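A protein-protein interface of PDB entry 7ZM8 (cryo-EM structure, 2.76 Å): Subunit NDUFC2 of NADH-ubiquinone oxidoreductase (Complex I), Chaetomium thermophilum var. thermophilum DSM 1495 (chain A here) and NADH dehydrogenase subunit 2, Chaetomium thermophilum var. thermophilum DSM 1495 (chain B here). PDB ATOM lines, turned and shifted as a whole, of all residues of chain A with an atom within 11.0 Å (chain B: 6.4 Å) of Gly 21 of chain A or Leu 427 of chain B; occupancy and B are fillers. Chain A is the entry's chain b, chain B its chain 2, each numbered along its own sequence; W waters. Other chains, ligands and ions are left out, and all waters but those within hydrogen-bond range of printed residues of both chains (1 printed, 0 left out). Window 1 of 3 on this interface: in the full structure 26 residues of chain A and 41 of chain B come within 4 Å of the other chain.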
ATOM      1  N   LEU A  13       7.988 -27.363  26.200  1.00  0.00           N
ATOM      2  CA  LEU A  13       7.313 -26.213  26.787  1.00  0.00           C
ATOM      3  C   LEU A  13       5.861 -26.136  26.333  1.00  0.00           C
ATOM      4  O   LEU A  13       4.971 -25.811  27.126  1.00  0.00           O
ATOM      5  CB  LEU A  13       8.050 -24.930  26.421  1.00  0.00           C
ATOM      6  CG  LEU A  13       9.460 -24.741  26.966  1.00  0.00           C
ATOM      7  CD1 LEU A  13       9.872 -23.294  26.805  1.00  0.00           C
ATOM      8  CD2 LEU A  13       9.549 -25.177  28.418  1.00  0.00           C
ATOM      9  N   ALA A  14       5.606 -26.422  25.056  1.00  0.00           N
ATOM     10  CA  ALA A  14       4.245 -26.355  24.539  1.00  0.00           C
ATOM     11  C   ALA A  14       3.378 -27.485  25.071  1.00  0.00           C
ATOM     12  O   ALA A  14       2.162 -27.318  25.196  1.00  0.00           O
ATOM     13  CB  ALA A  14       4.265 -26.369  23.012  1.00  0.00           C
ATOM     14  N   VAL A  15       3.975 -28.636  25.381  1.00  0.00           N
ATOM     15  CA  VAL A  15       3.201 -29.746  25.925  1.00  0.00           C
ATOM     16  C   VAL A  15       2.742 -29.431  27.342  1.00  0.00           C
ATOM     17  O   VAL A  15       1.614 -29.751  27.728  1.00  0.00           O
ATOM     18  CB  VAL A  15       4.019 -31.050  25.856  1.00  0.00           C
ATOM     19  CG1 VAL A  15       3.386 -32.136  26.708  1.00  0.00           C
ATOM     20  CG2 VAL A  15       4.135 -31.517  24.421  1.00  0.00           C
ATOM     21  N   ARG A  16       3.603 -28.796  28.136  1.00  0.00           N
ATOM     22  CA  ARG A  16       3.200 -28.378  29.472  1.00  0.00           C
ATOM     23  C   ARG A  16       2.077 -27.352  29.407  1.00  0.00           C
ATOM     24  O   ARG A  16       1.126 -27.410  30.195  1.00  0.00           O
ATOM     25  CB  ARG A  16       4.405 -27.820  30.227  1.00  0.00           C
ATOM     26  CG  ARG A  16       4.147 -27.481  31.678  1.00  0.00           C
ATOM     27  CD  ARG A  16       3.529 -28.630  32.414  1.00  0.00           C
ATOM     28  NE  ARG A  16       3.203 -28.265  33.780  1.00  0.00           N
ATOM     29  CZ  ARG A  16       2.750 -29.115  34.690  1.00  0.00           C
ATOM     30  NH1 ARG A  16       2.479 -28.694  35.915  1.00  0.00           N
ATOM     31  NH2 ARG A  16       2.572 -30.383  34.371  1.00  0.00           N
ATOM     32  N   PHE A  17       2.167 -26.409  28.469  1.00  0.00           N
ATOM     33  CA  PHE A  17       1.130 -25.394  28.316  1.00  0.00           C
ATOM     34  C   PHE A  17      -0.194 -26.010  27.901  1.00  0.00           C
ATOM     35  O   PHE A  17      -1.251 -25.629  28.414  1.00  0.00           O
ATOM     36  CB  PHE A  17       1.568 -24.356  27.291  1.00  0.00           C
ATOM     37  CG  PHE A  17       2.349 -23.231  27.877  1.00  0.00           C
ATOM     38  CD1 PHE A  17       1.752 -22.341  28.744  1.00  0.00           C
ATOM     39  CD2 PHE A  17       3.688 -23.068  27.568  1.00  0.00           C
ATOM     40  CE1 PHE A  17       2.472 -21.313  29.284  1.00  0.00           C
ATOM     41  CE2 PHE A  17       4.415 -22.038  28.110  1.00  0.00           C
ATOM     42  CZ  PHE A  17       3.810 -21.162  28.968  1.00  0.00           C
ATOM     43  N   TRP A  18      -0.157 -26.956  26.963  1.00  0.00           N
ATOM     44  CA  TRP A  18      -1.378 -27.603  26.500  1.00  0.00           C
ATOM     45  C   TRP A  18      -1.972 -28.506  27.568  1.00  0.00           C
ATOM     46  O   TRP A  18      -3.196 -28.610  27.675  1.00  0.00           O
ATOM     47  CB  TRP A  18      -1.095 -28.400  25.230  1.00  0.00           C
ATOM     48  CG  TRP A  18      -1.459 -27.689  23.979  1.00  0.00           C
ATOM     49  CD1 TRP A  18      -0.688 -26.810  23.283  1.00  0.00           C
ATOM     50  CD2 TRP A  18      -2.692 -27.793  23.265  1.00  0.00           C
ATOM     51  NE1 TRP A  18      -1.364 -26.356  22.180  1.00  0.00           N
ATOM     52  CE2 TRP A  18      -2.600 -26.944  22.148  1.00  0.00           C
ATOM     53  CE3 TRP A  18      -3.865 -28.519  23.461  1.00  0.00           C
ATOM     54  CZ2 TRP A  18      -3.633 -26.807  21.233  1.00  0.00           C
ATOM     55  CZ3 TRP A  18      -4.887 -28.374  22.553  1.00  0.00           C
ATOM     56  CH2 TRP A  18      -4.766 -27.530  21.453  1.00  0.00           C
ATOM     57  N   GLN A  19      -1.125 -29.164  28.358  1.00  0.00           N
ATOM     58  CA  GLN A  19      -1.605 -30.011  29.444  1.00  0.00           C
ATOM     59  C   GLN A  19      -2.467 -29.230  30.422  1.00  0.00           C
ATOM     60  O   GLN A  19      -3.577 -29.648  30.761  1.00  0.00           O
ATOM     61  CB  GLN A  19      -0.424 -30.623  30.184  1.00  0.00           C
ATOM     62  CG  GLN A  19      -0.832 -31.630  31.210  1.00  0.00           C
ATOM     63  CD  GLN A  19       0.069 -31.613  32.413  1.00  0.00           C
ATOM     64  OE1 GLN A  19       1.280 -31.471  32.293  1.00  0.00           O
ATOM     65  NE2 GLN A  19      -0.522 -31.733  33.589  1.00  0.00           N
ATOM     66  N   LEU A  20      -1.961 -28.094  30.898  1.00  0.00           N
ATOM     67  CA  LEU A  20      -2.700 -27.314  31.878  1.00  0.00           C
ATOM     68  C   LEU A  20      -3.944 -26.693  31.266  1.00  0.00           C
ATOM     69  O   LEU A  20      -4.954 -26.535  31.955  1.00  0.00           O
ATOM     70  CB  LEU A  20      -1.788 -26.250  32.482  1.00  0.00           C
ATOM     71  CG  LEU A  20      -0.473 -26.794  33.056  1.00  0.00           C
ATOM     72  CD1 LEU A  20       0.405 -25.693  33.610  1.00  0.00           C
ATOM     73  CD2 LEU A  20      -0.747 -27.837  34.110  1.00  0.00           C
ATOM     74  N   GLY A  21      -3.895 -26.354  29.977  1.00  0.00           N
ATOM     75  CA  GLY A  21      -5.086 -25.863  29.305  1.00  0.00           C
ATOM     76  C   GLY A  21      -6.180 -26.910  29.217  1.00  0.00           C
ATOM     77  O   GLY A  21      -7.348 -26.617  29.468  1.00  0.00           O
ATOM     78  N   ILE A  22      -5.830 -28.161  28.925  1.00  0.00           N
ATOM     79  CA  ILE A  22      -6.833 -29.271  28.917  1.00  0.00           C
ATOM     80  C   ILE A  22      -7.409 -29.489  30.312  1.00  0.00           C
ATOM     81  O   ILE A  22      -8.634 -29.595  30.428  1.00  0.00           O
ATOM     82  CB  ILE A  22      -6.224 -30.546  28.316  1.00  0.00           C
ATOM     83  CG1 ILE A  22      -5.960 -30.376  26.818  1.00  0.00           C
ATOM     84  CG2 ILE A  22      -7.092 -31.762  28.598  1.00  0.00           C
ATOM     85  CD1 ILE A  22      -4.916 -31.311  26.280  1.00  0.00           C
ATOM     86  N   GLU A  23      -6.548 -29.543  31.328  1.00  0.00           N
ATOM     87  CA  GLU A  23      -6.958 -29.754  32.738  1.00  0.00           C
ATOM     88  C   GLU A  23      -7.613 -28.483  33.260  1.00  0.00           C
ATOM     89  O   GLU A  23      -8.109 -28.518  34.377  1.00  0.00           O
ATOM     90  CB  GLU A  23      -5.720 -30.088  33.559  1.00  0.00           C
ATOM     91  CG  GLU A  23      -5.205 -31.494  33.365  1.00  0.00           C
ATOM     92  CD  GLU A  23      -4.152 -31.832  34.399  1.00  0.00           C
ATOM     93  OE1 GLU A  23      -3.725 -30.909  35.105  1.00  0.00           O
ATOM     94  OE2 GLU A  23      -3.773 -33.008  34.506  1.00  0.00           O
ATOM     95  N   MET A  24      -7.570 -27.400  32.491  1.00  0.00           N
ATOM     96  CA  MET A  24      -8.128 -26.077  32.881  1.00  0.00           C
ATOM     97  C   MET A  24      -7.528 -25.650  34.223  1.00  0.00           C
ATOM     98  O   MET A  24      -8.243 -25.076  35.043  1.00  0.00           O
ATOM     99  CB  MET A  24      -9.652 -26.033  32.820  1.00  0.00           C
ATOM    100  CG  MET A  24     -10.199 -26.521  31.504  1.00  0.00           C
ATOM    101  SD  MET A  24     -11.999 -26.576  31.475  1.00  0.00           S
ATOM    102  CE  MET A  24     -12.370 -24.835  31.277  1.00  0.00           C
ATOM    103  N   ARG A  25      -6.237 -25.902  34.403  1.00  0.00           N
ATOM    104  CA  ARG A  25      -5.500 -25.524  35.634  1.00  0.00           C
ATOM    105  C   ARG A  25      -4.806 -24.181  35.381  1.00  0.00           C
ATOM    106  O   ARG A  25      -4.697 -23.786  34.217  1.00  0.00           O
ATOM    107  CB  ARG A  25      -4.493 -26.625  35.963  1.00  0.00           C
ATOM    108  CG  ARG A  25      -4.886 -27.477  37.160  1.00  0.00           C
ATOM    109  CD  ARG A  25      -3.860 -28.558  37.408  1.00  0.00           C
ATOM    110  NE  ARG A  25      -2.540 -27.989  37.624  1.00  0.00           N
ATOM    111  CZ  ARG A  25      -1.418 -28.684  37.564  1.00  0.00           C
ATOM    112  NH1 ARG A  25      -0.258 -28.089  37.775  1.00  0.00           N
ATOM    113  NH2 ARG A  25      -1.463 -29.970  37.275  1.00  0.00           N
ATOM    114  N   PRO A  26      -4.366 -23.407  36.412  1.00  0.00           N
ATOM    115  CA  PRO A  26      -3.743 -22.109  36.159  1.00  0.00           C
ATOM    116  C   PRO A  26      -2.325 -22.192  35.580  1.00  0.00           C
ATOM    117  O   PRO A  26      -1.471 -22.759  36.211  1.00  0.00           O
ATOM    118  CB  PRO A  26      -3.627 -21.454  37.542  1.00  0.00           C
ATOM    119  CG  PRO A  26      -3.575 -22.608  38.510  1.00  0.00           C
ATOM    120  CD  PRO A  26      -4.424 -23.681  37.866  1.00  0.00           C
ATOM    121  N   PHE A  27      -2.104 -21.642  34.389  1.00  0.00           N
ATOM    122  CA  PHE A  27      -0.712 -21.603  33.883  1.00  0.00           C
ATOM    123  C   PHE A  27       0.064 -20.670  34.809  1.00  0.00           C
ATOM    124  O   PHE A  27      -0.535 -19.656  35.215  1.00  0.00           O
ATOM    125  CB  PHE A  27      -0.641 -20.953  32.501  1.00  0.00           C
ATOM    126  CG  PHE A  27      -1.597 -21.447  31.448  1.00  0.00           C
ATOM    127  CD1 PHE A  27      -1.555 -22.757  31.003  1.00  0.00           C
ATOM    128  CD2 PHE A  27      -2.501 -20.580  30.858  1.00  0.00           C
ATOM    129  CE1 PHE A  27      -2.427 -23.193  30.018  1.00  0.00           C
ATOM    130  CE2 PHE A  27      -3.371 -21.018  29.873  1.00  0.00           C
ATOM    131  CZ  PHE A  27      -3.331 -22.326  29.453  1.00  0.00           C
ATOM    132  N   PHE A  28       1.277 -21.028  35.216  1.00  0.00           N
ATOM    133  CA  PHE A  28       2.155 -20.094  35.986  1.00  0.00           C
ATOM    134  C   PHE A  28       1.933 -20.059  37.497  1.00  0.00           C
ATOM    135  O   PHE A  28       2.171 -18.993  38.076  1.00  0.00           O
ATOM    136  CB  PHE A  28       2.266 -18.700  35.361  1.00  0.00           C
ATOM    137  CG  PHE A  28       2.604 -18.697  33.894  1.00  0.00           C
ATOM    138  CD1 PHE A  28       3.726 -19.356  33.425  1.00  0.00           C
ATOM    139  CD2 PHE A  28       1.796 -18.036  32.985  1.00  0.00           C
ATOM    140  CE1 PHE A  28       4.032 -19.354  32.075  1.00  0.00           C
ATOM    141  CE2 PHE A  28       2.103 -18.035  31.635  1.00  0.00           C
ATOM    142  CZ  PHE A  28       3.223 -18.687  31.185  1.00  0.00           C
ATOM    143  N   TYR A  36       8.030 -26.561  33.953  1.00  0.00           N
ATOM    144  CA  TYR A  36       8.478 -26.016  32.674  1.00  0.00           C
ATOM    145  C   TYR A  36       9.934 -26.346  32.370  1.00  0.00           C
ATOM    146  O   TYR A  36      10.217 -26.788  31.246  1.00  0.00           O
ATOM    147  CB  TYR A  36       8.210 -24.508  32.633  1.00  0.00           C
ATOM    148  CG  TYR A  36       6.755 -24.163  32.478  1.00  0.00           C
ATOM    149  CD1 TYR A  36       6.087 -24.423  31.298  1.00  0.00           C
ATOM    150  CD2 TYR A  36       6.048 -23.582  33.513  1.00  0.00           C
ATOM    151  CE1 TYR A  36       4.761 -24.109  31.150  1.00  0.00           C
ATOM    152  CE2 TYR A  36       4.721 -23.267  33.375  1.00  0.00           C
ATOM    153  CZ  TYR A  36       4.081 -23.531  32.191  1.00  0.00           C
ATOM    154  OH  TYR A  36       2.751 -23.218  32.052  1.00  0.00           O
ATOM    155  N   PHE A  39       9.792 -30.271  31.617  1.00  0.00           N
ATOM    156  CA  PHE A  39       9.223 -30.629  30.322  1.00  0.00           C
ATOM    157  C   PHE A  39      10.140 -30.208  29.186  1.00  0.00           C
ATOM    158  O   PHE A  39      10.355 -30.970  28.237  1.00  0.00           O
ATOM    159  CB  PHE A  39       7.847 -29.986  30.162  1.00  0.00           C
ATOM    160  CG  PHE A  39       6.727 -30.782  30.762  1.00  0.00           C
ATOM    161  CD1 PHE A  39       6.708 -31.072  32.113  1.00  0.00           C
ATOM    162  CD2 PHE A  39       5.687 -31.227  29.977  1.00  0.00           C
ATOM    163  CE1 PHE A  39       5.683 -31.792  32.660  1.00  0.00           C
ATOM    164  CE2 PHE A  39       4.657 -31.944  30.525  1.00  0.00           C
ATOM    165  CZ  PHE A  39       4.657 -32.229  31.866  1.00  0.00           C
ATOM    166  N   PHE B 422     -17.183 -26.973  23.695  1.00  0.00           N
ATOM    167  CA  PHE B 422     -16.248 -25.821  23.604  1.00  0.00           C
ATOM    168  C   PHE B 422     -16.396 -24.975  24.868  1.00  0.00           C
ATOM    169  O   PHE B 422     -15.383 -24.525  25.420  1.00  0.00           O
ATOM    170  CB  PHE B 422     -16.533 -25.031  22.326  1.00  0.00           C
ATOM    171  CG  PHE B 422     -15.779 -23.736  22.176  1.00  0.00           C
ATOM    172  CD1 PHE B 422     -14.395 -23.720  22.128  1.00  0.00           C
ATOM    173  CD2 PHE B 422     -16.459 -22.535  22.058  1.00  0.00           C
ATOM    174  CE1 PHE B 422     -13.708 -22.527  21.977  1.00  0.00           C
ATOM    175  CE2 PHE B 422     -15.770 -21.342  21.910  1.00  0.00           C
ATOM    176  CZ  PHE B 422     -14.398 -21.342  21.864  1.00  0.00           C
ATOM    177  N   ASN B 425     -14.962 -27.256  27.959  1.00  0.00           N
ATOM    178  CA  ASN B 425     -13.485 -27.467  27.945  1.00  0.00           C
ATOM    179  C   ASN B 425     -12.928 -27.016  26.580  1.00  0.00           C
ATOM    180  O   ASN B 425     -12.980 -27.831  25.649  1.00  0.00           O
ATOM    181  CB  ASN B 425     -13.099 -28.895  28.332  1.00  0.00           C
ATOM    182  CG  ASN B 425     -11.667 -29.034  28.806  1.00  0.00           C
ATOM    183  OD1 ASN B 425     -10.787 -28.296  28.379  1.00  0.00           O
ATOM    184  ND2 ASN B 425     -11.424 -29.995  29.682  1.00  0.00           N
ATOM    185  N   PRO B 426     -12.415 -25.768  26.400  1.00  0.00           N
ATOM    186  CA  PRO B 426     -11.998 -25.283  25.079  1.00  0.00           C
ATOM    187  C   PRO B 426     -10.816 -26.011  24.454  1.00  0.00           C
ATOM    188  O   PRO B 426     -10.887 -26.355  23.274  1.00  0.00           O
ATOM    189  CB  PRO B 426     -11.658 -23.813  25.345  1.00  0.00           C
ATOM    190  CG  PRO B 426     -12.365 -23.481  26.589  1.00  0.00           C
ATOM    191  CD  PRO B 426     -12.376 -24.701  27.406  1.00  0.00           C
ATOM    192  N   LEU B 427      -9.726 -26.241  25.185  1.00  0.00           N
ATOM    193  CA  LEU B 427      -8.600 -26.926  24.558  1.00  0.00           C
ATOM    194  C   LEU B 427      -8.841 -28.411  24.351  1.00  0.00           C
ATOM    195  O   LEU B 427      -8.290 -28.984  23.407  1.00  0.00           O
ATOM    196  CB  LEU B 427      -7.300 -26.740  25.341  1.00  0.00           C
ATOM    197  CG  LEU B 427      -6.519 -25.451  25.127  1.00  0.00           C
ATOM    198  CD1 LEU B 427      -7.184 -24.260  25.780  1.00  0.00           C
ATOM    199  CD2 LEU B 427      -5.096 -25.642  25.597  1.00  0.00           C
ATOM    200  N   LEU B 428      -9.622 -29.062  25.211  1.00  0.00           N
ATOM    201  CA  LEU B 428     -10.020 -30.427  24.899  1.00  0.00           C
ATOM    202  C   LEU B 428     -10.859 -30.456  23.631  1.00  0.00           C
ATOM    203  O   LEU B 428     -10.702 -31.349  22.792  1.00  0.00           O
ATOM    204  CB  LEU B 428     -10.778 -31.048  26.069  1.00  0.00           C
ATOM    205  CG  LEU B 428     -10.824 -32.582  26.075  1.00  0.00           C
ATOM    206  CD1 LEU B 428      -9.444 -33.179  25.833  1.00  0.00           C
ATOM    207  CD2 LEU B 428     -11.413 -33.105  27.365  1.00  0.00           C
ATOM    208  N   SER B 429     -11.744 -29.473  23.472  1.00  0.00           N
ATOM    209  CA  SER B 429     -12.509 -29.334  22.238  1.00  0.00           C
ATOM    210  C   SER B 429     -11.599 -29.052  21.054  1.00  0.00           C
ATOM    211  O   SER B 429     -11.810 -29.581  19.959  1.00  0.00           O
ATOM    212  CB  SER B 429     -13.526 -28.212  22.389  1.00  0.00           C
ATOM    213  OG  SER B 429     -14.471 -28.527  23.387  1.00  0.00           O
ATOM    214  N   LEU B 430     -10.563 -28.251  21.238  1.00  0.00           N
ATOM    215  CA  LEU B 430      -9.670 -27.877  20.120  1.00  0.00           C
ATOM    216  C   LEU B 430      -8.750 -29.039  19.810  1.00  0.00           C
ATOM    217  O   LEU B 430      -8.358 -29.156  18.672  1.00  0.00           O
ATOM    218  CB  LEU B 430      -8.889 -26.625  20.521  1.00  0.00           C
ATOM    219  CG  LEU B 430      -8.095 -25.947  19.409  1.00  0.00           C
ATOM    220  CD1 LEU B 430      -9.031 -25.334  18.379  1.00  0.00           C
ATOM    221  CD2 LEU B 430      -7.171 -24.889  19.986  1.00  0.00           C
ATOM    222  N   SER B 431      -8.408 -29.846  20.806  1.00  0.00           N
ATOM    223  CA  SER B 431      -7.637 -31.050  20.528  1.00  0.00           C
ATOM    224  C   SER B 431      -8.420 -32.013  19.653  1.00  0.00           C
ATOM    225  O   SER B 431      -7.874 -32.587  18.705  1.00  0.00           O
ATOM    226  CB  SER B 431      -7.252 -31.730  21.836  1.00  0.00           C
ATOM    227  OG  SER B 431      -6.487 -30.877  22.650  1.00  0.00           O
ATOM    228  N   LEU B 432      -9.698 -32.219  19.966  1.00  0.00           N
ATOM    229  CA  LEU B 432     -10.541 -33.060  19.130  1.00  0.00           C
ATOM    230  C   LEU B 432     -10.766 -32.430  17.765  1.00  0.00           C
ATOM    231  O   LEU B 432     -10.912 -33.145  16.769  1.00  0.00           O
ATOM    232  CB  LEU B 432     -11.874 -33.322  19.826  1.00  0.00           C
ATOM    233  CG  LEU B 432     -12.803 -34.333  19.155  1.00  0.00           C
ATOM    234  CD1 LEU B 432     -12.099 -35.662  18.932  1.00  0.00           C
ATOM    235  CD2 LEU B 432     -14.050 -34.517  19.978  1.00  0.00           C
ATOM    236  N   ILE B 540      -2.676 -36.668  25.587  1.00  0.00           N
ATOM    237  CA  ILE B 540      -3.436 -35.917  24.592  1.00  0.00           C
ATOM    238  C   ILE B 540      -2.620 -34.740  24.082  1.00  0.00           C
ATOM    239  O   ILE B 540      -2.615 -34.436  22.884  1.00  0.00           O
ATOM    240  CB  ILE B 540      -4.778 -35.454  25.187  1.00  0.00           C
ATOM    241  CG1 ILE B 540      -5.749 -36.630  25.299  1.00  0.00           C
ATOM    242  CG2 ILE B 540      -5.370 -34.331  24.355  1.00  0.00           C
ATOM    243  CD1 ILE B 540      -6.912 -36.369  26.218  1.00  0.00           C
ATOM    244  N   THR B 544      -1.574 -34.211  20.015  1.00  0.00           N
ATOM    245  CA  THR B 544      -2.117 -33.033  19.351  1.00  0.00           C
ATOM    246  C   THR B 544      -1.001 -32.145  18.818  1.00  0.00           C
ATOM    247  O   THR B 544      -1.112 -31.581  17.724  1.00  0.00           O
ATOM    248  CB  THR B 544      -3.019 -32.273  20.329  1.00  0.00           C
ATOM    249  OG1 THR B 544      -4.216 -33.023  20.548  1.00  0.00           O
ATOM    250  CG2 THR B 544      -3.391 -30.893  19.806  1.00  0.00           C
HETATM  251  O   HOH W   1      -9.544 -25.964  28.013  1.00  0.00           O
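The side-chain hydroxyl (OG) of Ser 429 of chain B lies within hydrogen-bond range of the backbone carbonyl oxygen (O) of Asn 425 of chain B.
The backbone carbonyl oxygen of Leu 427 of chain B lies within hydrogen-bond range of the side-chain hydroxyl of Ser 431 of chain B (2.7 Å).
The side-chain hydroxyl (OG1) of Thr 544 of chain B sits at hydrogen-bond distance from the backbone carbonyl oxygen (O) of Ile 540 of chain B, at 3.2 Å.
The side-chain amide oxygen (OD1) of Asn 425 of chain B sits at hydrogen-bond distance from the backbone NH (N) of Leu 428 of chain B.
CZ3 of Trp 18 of chain A touches O of Leu 427 of chain B, at 3.6 Å.
Trp 18 of chain A touches Leu 430 of chain B.
OG of Ser 431 of chain B touches CZ3 of Trp 18 of chain A, at 3.0 Å.
CH2 of Trp 18 of chain A touches CG2 of Thr 544 of chain B (3.99 Å).
O of Gly 21 of chain A touches OD1 of Asn 425 of chain B, at 3.98 Å.
Gly 21 of chain A touches Leu 427 of chain B.
Ile 22 of chain A touches Leu 428 of chain B (CG2 to CD1, 3.9 Å).
Ser 431 of chain B touches Ile 22 of chain A (OG to CD1, 3.98 Å).
CD1 of Ile 22 of chain A touches CG2 of Ile 540 of chain B, 3.6 Å away.
Met 24 of chain A touches Pro 426 of chain B (CE to CD, 3.9 Å).
Water W1 lies within hydrogen-bond range of the side-chain amide oxygen (OD1) of Asn 425 of chain B (2.7 Å), the backbone carbonyl oxygen (O) of Gly 21 of chain A (2.7 Å) and the backbone NH (N) of Leu 427 of chain B (2.8 Å).
Of the 11 printed residues of chain B, 8 touch a printed residue of chain A.
Hydrophobic or aromatic side chains of chain B within 4 Å of the printed part of chain A: Pro 426, Leu 427, Leu 428, Leu 430 and Ile 540.
Along chain B the printed residues that touch a printed residue of chain A span positions 425 to 544.
Of the 18 printed residues of chain A, 4 touch a printed residue of chain B.
Printed residues of chain A that touch a printed residue of chain B: Trp 18, Gly 21, Ile 22 and Met 24.
OD1 of Asn 425 of chain B sits close to SD of Met 24 of chain A (3.7 Å).
O of Ile 22 of chain A is in hydrogen-bond range of ND2 of Asn 425 of chain B (2.9 Å).
Gly 21 of chain A touches just these residues of chain B: Asn 425 and Leu 427.
Printed residues of chain A within 4 Å of Leu 427 of chain B: Trp 18 (3.6 Å) and Gly 21 (3.7 Å).
Of the printed residues of chain A, Asn 425 of chain B touches Gly 21, Ile 22 and Met 24.
Pro 426 of chain B touches just one residue of chain A: Met 24 (3.9 Å).
Of chain A, only Ile 22 comes within 4 Å of Leu 428 of chain B.
Ser 429 of chain B touches none of the printed residues of chain A.
Leu 430 of chain B touches just one residue of chain A: Trp 18 (3.9 Å).
Ser 431 of chain B touches just these residues of chain A: Trp 18 and Ile 22.
Printed residues of chain A within 4 Å of Thr 544 of chain B: Trp 18.
Printed residues of chain B within 4 Å of Met 24 of chain A: Asn 425 (3.6 Å) and Pro 426 (3.9 Å).
Of the printed residues of chain A, Ile 540 of chain B touches Ile 22.
Of the printed residues of chain B, Ile 22 of chain A touches Asn 425, Leu 428, Ser 431 and Ile 540.
Of the printed residues of chain B, Trp 18 of chain A touches Leu 427 (3.6 Å), Leu 430 (3.9 Å), Ser 431 (3.0 Å) and Thr 544 (3.99 Å).
The nearest printed residue of chain B that does not touch Trp 18 of chain A is Leu 428 of chain B (5.5 Å).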
